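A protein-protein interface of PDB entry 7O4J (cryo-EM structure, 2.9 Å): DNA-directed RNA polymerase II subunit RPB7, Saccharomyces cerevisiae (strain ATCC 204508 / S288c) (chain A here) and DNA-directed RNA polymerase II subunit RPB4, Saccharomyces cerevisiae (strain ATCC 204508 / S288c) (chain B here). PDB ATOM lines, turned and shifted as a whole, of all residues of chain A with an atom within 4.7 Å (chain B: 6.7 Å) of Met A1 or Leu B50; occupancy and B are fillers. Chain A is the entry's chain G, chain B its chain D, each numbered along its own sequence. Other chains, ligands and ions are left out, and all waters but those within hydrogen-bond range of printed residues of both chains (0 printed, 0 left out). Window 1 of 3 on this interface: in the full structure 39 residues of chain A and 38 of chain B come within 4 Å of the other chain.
The backbone NH (N) of Ile A4 lies within hydrogen-bond range of the backbone carbonyl oxygen (O) of Ile B48, at 3.2 Å. The backbone carbonyl oxygen (O) of Phe A2 is in hydrogen-bond range of the backbone NH (N) of Leu B50, at 2.7 Å. The side-chain sulfur (SD) of Met A1 sits close to the backbone carbonyl oxygen (O) of Leu B50 (3.7 Å).
Of chain B, only Leu B50, Phe B175, Ala B178 and Gln B179 come within 4 Å of Met A1. Of chain A, only Met A1 (3.7 Å), Phe A2 (2.7 Å) and Ile A4 (3.7 Å) come within 4 Å of Leu B50. Of the printed residues of chain B, Val A77 touches Val B58. Of the printed residues of chain B, Phe A3 touches Phe B33 (3.4 Å), Leu B47 (3.4 Å) and Ile B48 (3.2 Å). Printed residues of chain B within 4 Å of Lys A80: Phe B33. Ser B53 touches none of the printed residues of chain A. Pro B174 touches none of the printed residues of chain A. The nearest residue of chain B that does not touch Met A1 is Ala B49 (4.4 Å). The nearest residue of chain A that does not touch Leu B50 is Val A77 (4.4 Å). The nearest printed residue of chain B that does not touch Lys A80 is Phe B175 (6.4 Å).
Printed residues of chain A that touch a printed residue of chain B: Met A1, Phe A2, Phe A3, Ile A4, Val A77, Lys A80 and Glu A85. Among the printed residues, no Asp or Glu carboxylate lies within 4 Å of a Lys or Arg side-chain nitrogen of the other chain.
The side-chain hydroxyl of Ser B182 lies within hydrogen-bond range of the backbone NH of Leu B52 (3.4 Å). O of Ala B178 sits at hydrogen-bond distance from OG of Ser B182 (2.5 Å). The backbone carbonyl oxygen of Met A1 is in hydrogen-bond range of the backbone NH of Lys A80, at 3.0 Å. The backbone carbonyl oxygen (O) of Phe A3 lies within hydrogen-bond range of the backbone NH (N) of Val A78, at 2.9 Å.
Among the printed residues, merely in contact across the chains: Phe A3 with Ile B48 (3.2 Å), Phe A3 with Leu B47 (3.4 Å), Phe A3 with Phe B33 (3.4 Å), Glu A85 with Gln B179 (3.5 Å), Met A1 with Phe B175 (3.5 Å), Phe A2 with Ala B49 (3.5 Å), Glu A85 with Phe B175 (3.6 Å), Met A1 with Ala B178 (3.6 Å), Phe A2 with Leu B52 (3.6 Å), Lys A80 with Phe B33 (3.6 Å), Phe A2 with Ala B55 (3.7 Å), Met A1 with Gln B179 (3.7 Å), Ile A4 with Leu B50 (3.7 Å) and Val A77 with Val B58 (3.8 Å).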
ATOM      1  N   MET A   1     -24.721 -19.530  21.322  1.00  0.00           N
ATOM      2  CA  MET A   1     -23.763 -18.390  21.363  1.00  0.00           C
ATOM      3  C   MET A   1     -22.576 -18.657  20.446  1.00  0.00           C
ATOM      4  O   MET A   1     -22.090 -19.783  20.361  1.00  0.00           O
ATOM      5  CB  MET A   1     -23.281 -18.148  22.796  1.00  0.00           C
ATOM      6  CG  MET A   1     -22.354 -16.951  22.950  1.00  0.00           C
ATOM      7  SD  MET A   1     -23.087 -15.406  22.384  1.00  0.00           S
ATOM      8  CE  MET A   1     -24.021 -14.930  23.834  1.00  0.00           C
ATOM      9  N   PHE A   2     -22.112 -17.612  19.767  1.00  0.00           N
ATOM     10  CA  PHE A   2     -20.997 -17.709  18.835  1.00  0.00           C
ATOM     11  C   PHE A   2     -19.735 -17.185  19.509  1.00  0.00           C
ATOM     12  O   PHE A   2     -19.715 -16.052  20.003  1.00  0.00           O
ATOM     13  CB  PHE A   2     -21.285 -16.921  17.557  1.00  0.00           C
ATOM     14  CG  PHE A   2     -22.373 -17.513  16.712  1.00  0.00           C
ATOM     15  CD1 PHE A   2     -23.704 -17.283  17.013  1.00  0.00           C
ATOM     16  CD2 PHE A   2     -22.067 -18.298  15.614  1.00  0.00           C
ATOM     17  CE1 PHE A   2     -24.707 -17.826  16.237  1.00  0.00           C
ATOM     18  CE2 PHE A   2     -23.066 -18.844  14.835  1.00  0.00           C
ATOM     19  CZ  PHE A   2     -24.387 -18.608  15.146  1.00  0.00           C
ATOM     20  N   PHE A   3     -18.693 -18.010  19.532  1.00  0.00           N
ATOM     21  CA  PHE A   3     -17.396 -17.634  20.070  1.00  0.00           C
ATOM     22  C   PHE A   3     -16.322 -17.798  19.004  1.00  0.00           C
ATOM     23  O   PHE A   3     -16.463 -18.595  18.072  1.00  0.00           O
ATOM     24  CB  PHE A   3     -17.021 -18.486  21.286  1.00  0.00           C
ATOM     25  CG  PHE A   3     -18.080 -18.540  22.349  1.00  0.00           C
ATOM     26  CD1 PHE A   3     -19.060 -19.515  22.319  1.00  0.00           C
ATOM     27  CD2 PHE A   3     -18.081 -17.629  23.390  1.00  0.00           C
ATOM     28  CE1 PHE A   3     -20.028 -19.572  23.299  1.00  0.00           C
ATOM     29  CE2 PHE A   3     -19.047 -17.683  24.372  1.00  0.00           C
ATOM     30  CZ  PHE A   3     -20.019 -18.655  24.327  1.00  0.00           C
ATOM     31  N   ILE A   4     -15.244 -17.036  19.151  1.00  0.00           N
ATOM     32  CA  ILE A   4     -14.030 -17.225  18.369  1.00  0.00           C
ATOM     33  C   ILE A   4     -13.031 -17.923  19.280  1.00  0.00           C
ATOM     34  O   ILE A   4     -12.562 -17.343  20.264  1.00  0.00           O
ATOM     35  CB  ILE A   4     -13.480 -15.896  17.836  1.00  0.00           C
ATOM     36  CG1 ILE A   4     -14.276 -15.461  16.604  1.00  0.00           C
ATOM     37  CG2 ILE A   4     -11.999 -16.026  17.501  1.00  0.00           C
ATOM     38  CD1 ILE A   4     -13.958 -14.061  16.124  1.00  0.00           C
ATOM     39  N   VAL A  77     -14.588 -20.199  14.436  1.00  0.00           N
ATOM     40  CA  VAL A  77     -15.842 -19.704  14.990  1.00  0.00           C
ATOM     41  C   VAL A  77     -16.684 -20.917  15.355  1.00  0.00           C
ATOM     42  O   VAL A  77     -16.989 -21.751  14.494  1.00  0.00           O
ATOM     43  CB  VAL A  77     -16.579 -18.797  13.992  1.00  0.00           C
ATOM     44  CG1 VAL A  77     -18.029 -18.607  14.410  1.00  0.00           C
ATOM     45  CG2 VAL A  77     -15.874 -17.457  13.869  1.00  0.00           C
ATOM     46  N   VAL A  78     -17.059 -21.022  16.627  1.00  0.00           N
ATOM     47  CA  VAL A  78     -17.762 -22.190  17.142  1.00  0.00           C
ATOM     48  C   VAL A  78     -19.024 -21.736  17.859  1.00  0.00           C
ATOM     49  O   VAL A  78     -19.009 -20.748  18.601  1.00  0.00           O
ATOM     50  CB  VAL A  78     -16.869 -23.018  18.090  1.00  0.00           C
ATOM     51  CG1 VAL A  78     -15.580 -23.415  17.389  1.00  0.00           C
ATOM     52  CG2 VAL A  78     -16.573 -22.242  19.364  1.00  0.00           C
ATOM     53  N   PHE A  79     -20.116 -22.462  17.635  1.00  0.00           N
ATOM     54  CA  PHE A  79     -21.383 -22.220  18.315  1.00  0.00           C
ATOM     55  C   PHE A  79     -21.515 -23.209  19.466  1.00  0.00           C
ATOM     56  O   PHE A  79     -21.563 -24.423  19.243  1.00  0.00           O
ATOM     57  CB  PHE A  79     -22.558 -22.362  17.347  1.00  0.00           C
ATOM     58  CG  PHE A  79     -23.902 -22.189  17.997  1.00  0.00           C
ATOM     59  CD1 PHE A  79     -24.537 -23.260  18.605  1.00  0.00           C
ATOM     60  CD2 PHE A  79     -24.530 -20.955  18.002  1.00  0.00           C
ATOM     61  CE1 PHE A  79     -25.770 -23.103  19.205  1.00  0.00           C
ATOM     62  CE2 PHE A  79     -25.765 -20.795  18.599  1.00  0.00           C
ATOM     63  CZ  PHE A  79     -26.385 -21.871  19.201  1.00  0.00           C
ATOM     64  N   LYS A  80     -21.580 -22.689  20.688  1.00  0.00           N
ATOM     65  CA  LYS A  80     -21.704 -23.510  21.887  1.00  0.00           C
ATOM     66  C   LYS A  80     -22.991 -23.146  22.616  1.00  0.00           C
ATOM     67  O   LYS A  80     -23.144 -21.989  23.043  1.00  0.00           O
ATOM     68  CB  LYS A  80     -20.498 -23.314  22.808  1.00  0.00           C
ATOM     69  CG  LYS A  80     -20.529 -24.160  24.076  1.00  0.00           C
ATOM     70  CD  LYS A  80     -20.348 -25.637  23.773  1.00  0.00           C
ATOM     71  CE  LYS A  80     -20.615 -26.492  24.998  1.00  0.00           C
ATOM     72  NZ  LYS A  80     -19.629 -26.240  26.081  1.00  0.00           N
ATOM     73  N   GLU A  85     -29.722 -19.871  28.469  1.00  0.00           N
ATOM     74  CA  GLU A  85     -29.573 -18.884  27.412  1.00  0.00           C
ATOM     75  C   GLU A  85     -30.818 -18.868  26.535  1.00  0.00           C
ATOM     76  O   GLU A  85     -31.465 -19.897  26.321  1.00  0.00           O
ATOM     77  CB  GLU A  85     -28.337 -19.184  26.563  1.00  0.00           C
ATOM     78  CG  GLU A  85     -28.045 -18.139  25.500  1.00  0.00           C
ATOM     79  CD  GLU A  85     -26.807 -18.462  24.688  1.00  0.00           C
ATOM     80  OE1 GLU A  85     -26.179 -19.509  24.950  1.00  0.00           O
ATOM     81  OE2 GLU A  85     -26.464 -17.670  23.787  1.00  0.00           O
ATOM     82  N   PHE B  33     -14.654 -22.013  28.300  1.00  0.00           N
ATOM     83  CA  PHE B  33     -15.217 -20.731  27.892  1.00  0.00           C
ATOM     84  C   PHE B  33     -15.133 -19.710  29.023  1.00  0.00           C
ATOM     85  O   PHE B  33     -16.063 -18.937  29.258  1.00  0.00           O
ATOM     86  CB  PHE B  33     -16.659 -20.903  27.423  1.00  0.00           C
ATOM     87  CG  PHE B  33     -16.784 -21.663  26.136  1.00  0.00           C
ATOM     88  CD1 PHE B  33     -16.739 -21.003  24.921  1.00  0.00           C
ATOM     89  CD2 PHE B  33     -16.937 -23.038  26.139  1.00  0.00           C
ATOM     90  CE1 PHE B  33     -16.851 -21.698  23.735  1.00  0.00           C
ATOM     91  CE2 PHE B  33     -17.047 -23.738  24.954  1.00  0.00           C
ATOM     92  CZ  PHE B  33     -17.004 -23.068  23.751  1.00  0.00           C
ATOM     93  N   LEU B  47     -12.555 -13.460  26.435  1.00  0.00           N
ATOM     94  CA  LEU B  47     -13.433 -14.341  25.679  1.00  0.00           C
ATOM     95  C   LEU B  47     -14.148 -13.549  24.593  1.00  0.00           C
ATOM     96  O   LEU B  47     -14.825 -12.557  24.879  1.00  0.00           O
ATOM     97  CB  LEU B  47     -14.442 -15.002  26.617  1.00  0.00           C
ATOM     98  CG  LEU B  47     -15.416 -15.997  25.980  1.00  0.00           C
ATOM     99  CD1 LEU B  47     -15.853 -17.037  26.998  1.00  0.00           C
ATOM    100  CD2 LEU B  47     -16.630 -15.293  25.386  1.00  0.00           C
ATOM    101  N   ILE B  48     -13.996 -13.988  23.347  1.00  0.00           N
ATOM    102  CA  ILE B  48     -14.597 -13.311  22.203  1.00  0.00           C
ATOM    103  C   ILE B  48     -15.974 -13.931  21.984  1.00  0.00           C
ATOM    104  O   ILE B  48     -16.095 -15.031  21.445  1.00  0.00           O
ATOM    105  CB  ILE B  48     -13.722 -13.420  20.955  1.00  0.00           C
ATOM    106  CG1 ILE B  48     -12.312 -12.891  21.235  1.00  0.00           C
ATOM    107  CG2 ILE B  48     -14.357 -12.662  19.797  1.00  0.00           C
ATOM    108  CD1 ILE B  48     -12.262 -11.434  21.661  1.00  0.00           C
ATOM    109  N   ALA B  49     -17.012 -13.219  22.406  1.00  0.00           N
ATOM    110  CA  ALA B  49     -18.391 -13.617  22.167  1.00  0.00           C
ATOM    111  C   ALA B  49     -18.997 -12.710  21.106  1.00  0.00           C
ATOM    112  O   ALA B  49     -18.894 -11.483  21.192  1.00  0.00           O
ATOM    113  CB  ALA B  49     -19.215 -13.548  23.453  1.00  0.00           C
ATOM    114  N   LEU B  50     -19.626 -13.319  20.106  1.00  0.00           N
ATOM    115  CA  LEU B  50     -20.154 -12.602  18.956  1.00  0.00           C
ATOM    116  C   LEU B  50     -21.674 -12.658  18.954  1.00  0.00           C
ATOM    117  O   LEU B  50     -22.267 -13.710  19.213  1.00  0.00           O
ATOM    118  CB  LEU B  50     -19.626 -13.191  17.645  1.00  0.00           C
ATOM    119  CG  LEU B  50     -18.129 -13.491  17.568  1.00  0.00           C
ATOM    120  CD1 LEU B  50     -17.839 -14.358  16.355  1.00  0.00           C
ATOM    121  CD2 LEU B  50     -17.322 -12.206  17.519  1.00  0.00           C
ATOM    122  N   ASN B  51     -22.299 -11.522  18.662  1.00  0.00           N
ATOM    123  CA  ASN B  51     -23.728 -11.500  18.409  1.00  0.00           C
ATOM    124  C   ASN B  51     -24.009 -12.025  17.002  1.00  0.00           C
ATOM    125  O   ASN B  51     -23.098 -12.278  16.210  1.00  0.00           O
ATOM    126  CB  ASN B  51     -24.286 -10.088  18.586  1.00  0.00           C
ATOM    127  CG  ASN B  51     -23.645  -9.084  17.652  1.00  0.00           C
ATOM    128  OD1 ASN B  51     -24.090  -8.898  16.521  1.00  0.00           O
ATOM    129  ND2 ASN B  51     -22.595  -8.423  18.126  1.00  0.00           N
ATOM    130  N   LEU B  52     -25.296 -12.191  16.693  1.00  0.00           N
ATOM    131  CA  LEU B  52     -25.668 -12.789  15.416  1.00  0.00           C
ATOM    132  C   LEU B  52     -25.148 -11.964  14.246  1.00  0.00           C
ATOM    133  O   LEU B  52     -24.628 -12.516  13.270  1.00  0.00           O
ATOM    134  CB  LEU B  52     -27.186 -12.940  15.331  1.00  0.00           C
ATOM    135  CG  LEU B  52     -27.815 -13.907  16.335  1.00  0.00           C
ATOM    136  CD1 LEU B  52     -29.328 -13.883  16.217  1.00  0.00           C
ATOM    137  CD2 LEU B  52     -27.285 -15.318  16.141  1.00  0.00           C
ATOM    138  N   SER B  53     -25.279 -10.639  14.323  1.00  0.00           N
ATOM    139  CA  SER B  53     -24.791  -9.790  13.241  1.00  0.00           C
ATOM    140  C   SER B  53     -23.272  -9.841  13.141  1.00  0.00           C
ATOM    141  O   SER B  53     -22.721  -9.952  12.039  1.00  0.00           O
ATOM    142  CB  SER B  53     -25.270  -8.355  13.450  1.00  0.00           C
ATOM    143  OG  SER B  53     -26.642  -8.331  13.801  1.00  0.00           O
ATOM    144  N   GLU B  54     -22.577  -9.758  14.277  1.00  0.00           N
ATOM    145  CA  GLU B  54     -21.121  -9.843  14.256  1.00  0.00           C
ATOM    146  C   GLU B  54     -20.658 -11.203  13.752  1.00  0.00           C
ATOM    147  O   GLU B  54     -19.715 -11.292  12.956  1.00  0.00           O
ATOM    148  CB  GLU B  54     -20.562  -9.571  15.652  1.00  0.00           C
ATOM    149  CG  GLU B  54     -19.123  -9.085  15.660  1.00  0.00           C
ATOM    150  CD  GLU B  54     -18.731  -8.446  16.979  1.00  0.00           C
ATOM    151  OE1 GLU B  54     -17.617  -7.886  17.061  1.00  0.00           O
ATOM    152  OE2 GLU B  54     -19.535  -8.504  17.932  1.00  0.00           O
ATOM    153  N   ALA B  55     -21.310 -12.277  14.204  1.00  0.00           N
ATOM    154  CA  ALA B  55     -20.938 -13.612  13.748  1.00  0.00           C
ATOM    155  C   ALA B  55     -21.152 -13.760  12.248  1.00  0.00           C
ATOM    156  O   ALA B  55     -20.332 -14.374  11.556  1.00  0.00           O
ATOM    157  CB  ALA B  55     -21.738 -14.667  14.511  1.00  0.00           C
ATOM    158  N   ARG B  56     -22.249 -13.206  11.729  1.00  0.00           N
ATOM    159  CA  ARG B  56     -22.508 -13.285  10.296  1.00  0.00           C
ATOM    160  C   ARG B  56     -21.398 -12.612   9.500  1.00  0.00           C
ATOM    161  O   ARG B  56     -20.917 -13.162   8.503  1.00  0.00           O
ATOM    162  CB  ARG B  56     -23.859 -12.645   9.979  1.00  0.00           C
ATOM    163  CG  ARG B  56     -24.473 -13.084   8.655  1.00  0.00           C
ATOM    164  CD  ARG B  56     -23.964 -12.260   7.478  1.00  0.00           C
ATOM    165  NE  ARG B  56     -24.107 -10.823   7.697  1.00  0.00           N
ATOM    166  CZ  ARG B  56     -25.224 -10.136   7.487  1.00  0.00           C
ATOM    167  NH1 ARG B  56     -26.318 -10.746   7.050  1.00  0.00           N
ATOM    168  NH2 ARG B  56     -25.249  -8.831   7.718  1.00  0.00           N
ATOM    169  N   VAL B  58     -18.258 -11.973  10.469  1.00  0.00           N
ATOM    170  CA  VAL B  58     -16.977 -12.651  10.637  1.00  0.00           C
ATOM    171  C   VAL B  58     -16.908 -13.896   9.763  1.00  0.00           C
ATOM    172  O   VAL B  58     -15.890 -14.158   9.112  1.00  0.00           O
ATOM    173  CB  VAL B  58     -16.748 -12.991  12.122  1.00  0.00           C
ATOM    174  CG1 VAL B  58     -15.607 -13.985  12.273  1.00  0.00           C
ATOM    175  CG2 VAL B  58     -16.467 -11.727  12.917  1.00  0.00           C
ATOM    176  N   ILE B  59     -17.983 -14.684   9.732  1.00  0.00           N
ATOM    177  CA  ILE B  59     -17.964 -15.930   8.974  1.00  0.00           C
ATOM    178  C   ILE B  59     -17.807 -15.647   7.485  1.00  0.00           C
ATOM    179  O   ILE B  59     -16.948 -16.229   6.814  1.00  0.00           O
ATOM    180  CB  ILE B  59     -19.231 -16.754   9.261  1.00  0.00           C
ATOM    181  CG1 ILE B  59     -19.222 -17.250  10.708  1.00  0.00           C
ATOM    182  CG2 ILE B  59     -19.330 -17.927   8.295  1.00  0.00           C
ATOM    183  CD1 ILE B  59     -20.555 -17.787  11.183  1.00  0.00           C
ATOM    184  N   PRO B 174     -18.716 -10.489  28.238  1.00  0.00           N
ATOM    185  CA  PRO B 174     -18.855 -10.704  26.788  1.00  0.00           C
ATOM    186  C   PRO B 174     -20.113 -11.470  26.414  1.00  0.00           C
ATOM    187  O   PRO B 174     -20.721 -11.190  25.374  1.00  0.00           O
ATOM    188  CB  PRO B 174     -17.584 -11.485  26.435  1.00  0.00           C
ATOM    189  CG  PRO B 174     -16.587 -11.043  27.439  1.00  0.00           C
ATOM    190  CD  PRO B 174     -17.354 -10.797  28.709  1.00  0.00           C
ATOM    191  N   PHE B 175     -20.517 -12.438  27.238  1.00  0.00           N
ATOM    192  CA  PHE B 175     -21.751 -13.169  26.972  1.00  0.00           C
ATOM    193  C   PHE B 175     -22.962 -12.246  27.014  1.00  0.00           C
ATOM    194  O   PHE B 175     -23.855 -12.341  26.164  1.00  0.00           O
ATOM    195  CB  PHE B 175     -21.905 -14.305  27.982  1.00  0.00           C
ATOM    196  CG  PHE B 175     -23.149 -15.124  27.792  1.00  0.00           C
ATOM    197  CD1 PHE B 175     -24.330 -14.769  28.421  1.00  0.00           C
ATOM    198  CD2 PHE B 175     -23.137 -16.250  26.988  1.00  0.00           C
ATOM    199  CE1 PHE B 175     -25.475 -15.520  28.248  1.00  0.00           C
ATOM    200  CE2 PHE B 175     -24.279 -17.005  26.813  1.00  0.00           C
ATOM    201  CZ  PHE B 175     -25.449 -16.640  27.444  1.00  0.00           C
ATOM    202  N   GLU B 176     -23.012 -11.346  28.000  1.00  0.00           N
ATOM    203  CA  GLU B 176     -24.166 -10.461  28.133  1.00  0.00           C
ATOM    204  C   GLU B 176     -24.259  -9.486  26.965  1.00  0.00           C
ATOM    205  O   GLU B 176     -25.339  -9.299  26.393  1.00  0.00           O
ATOM    206  CB  GLU B 176     -24.092  -9.703  29.457  1.00  0.00           C
ATOM    207  CG  GLU B 176     -23.993 -10.602  30.678  1.00  0.00           C
ATOM    208  CD  GLU B 176     -23.854  -9.820  31.969  1.00  0.00           C
ATOM    209  OE1 GLU B 176     -24.887  -9.377  32.513  1.00  0.00           O
ATOM    210  OE2 GLU B 176     -22.711  -9.647  32.440  1.00  0.00           O
ATOM    211  N   VAL B 177     -23.143  -8.856  26.597  1.00  0.00           N
ATOM    212  CA  VAL B 177     -23.165  -7.903  25.490  1.00  0.00           C
ATOM    213  C   VAL B 177     -23.552  -8.603  24.194  1.00  0.00           C
ATOM    214  O   VAL B 177     -24.320  -8.064  23.389  1.00  0.00           O
ATOM    215  CB  VAL B 177     -21.808  -7.186  25.364  1.00  0.00           C
ATOM    216  CG1 VAL B 177     -20.678  -8.184  25.185  1.00  0.00           C
ATOM    217  CG2 VAL B 177     -21.839  -6.214  24.198  1.00  0.00           C
ATOM    218  N   ALA B 178     -23.028  -9.810  23.968  1.00  0.00           N
ATOM    219  CA  ALA B 178     -23.412 -10.561  22.779  1.00  0.00           C
ATOM    220  C   ALA B 178     -24.900 -10.879  22.780  1.00  0.00           C
ATOM    221  O   ALA B 178     -25.535 -10.868  21.719  1.00  0.00           O
ATOM    222  CB  ALA B 178     -22.594 -11.848  22.686  1.00  0.00           C
ATOM    223  N   GLN B 179     -25.470 -11.168  23.951  1.00  0.00           N
ATOM    224  CA  GLN B 179     -26.903 -11.424  24.038  1.00  0.00           C
ATOM    225  C   GLN B 179     -27.713 -10.162  23.769  1.00  0.00           C
ATOM    226  O   GLN B 179     -28.752 -10.220  23.101  1.00  0.00           O
ATOM    227  CB  GLN B 179     -27.250 -11.993  25.414  1.00  0.00           C
ATOM    228  CG  GLN B 179     -27.003 -13.484  25.546  1.00  0.00           C
ATOM    229  CD  GLN B 179     -28.171 -14.313  25.053  1.00  0.00           C
ATOM    230  OE1 GLN B 179     -28.352 -14.500  23.850  1.00  0.00           O
ATOM    231  NE2 GLN B 179     -28.972 -14.818  25.983  1.00  0.00           N
ATOM    232  N   SER B 182     -28.036  -9.639  20.094  1.00  0.00           N
ATOM    233  CA  SER B 182     -28.692 -10.708  19.352  1.00  0.00           C
ATOM    234  C   SER B 182     -30.201 -10.729  19.532  1.00  0.00           C
ATOM    235  O   SER B 182     -30.917 -11.123  18.606  1.00  0.00           O
ATOM    236  CB  SER B 182     -28.125 -12.068  19.773  1.00  0.00           C
ATOM    237  OG  SER B 182     -26.709 -12.050  19.791  1.00  0.00           O
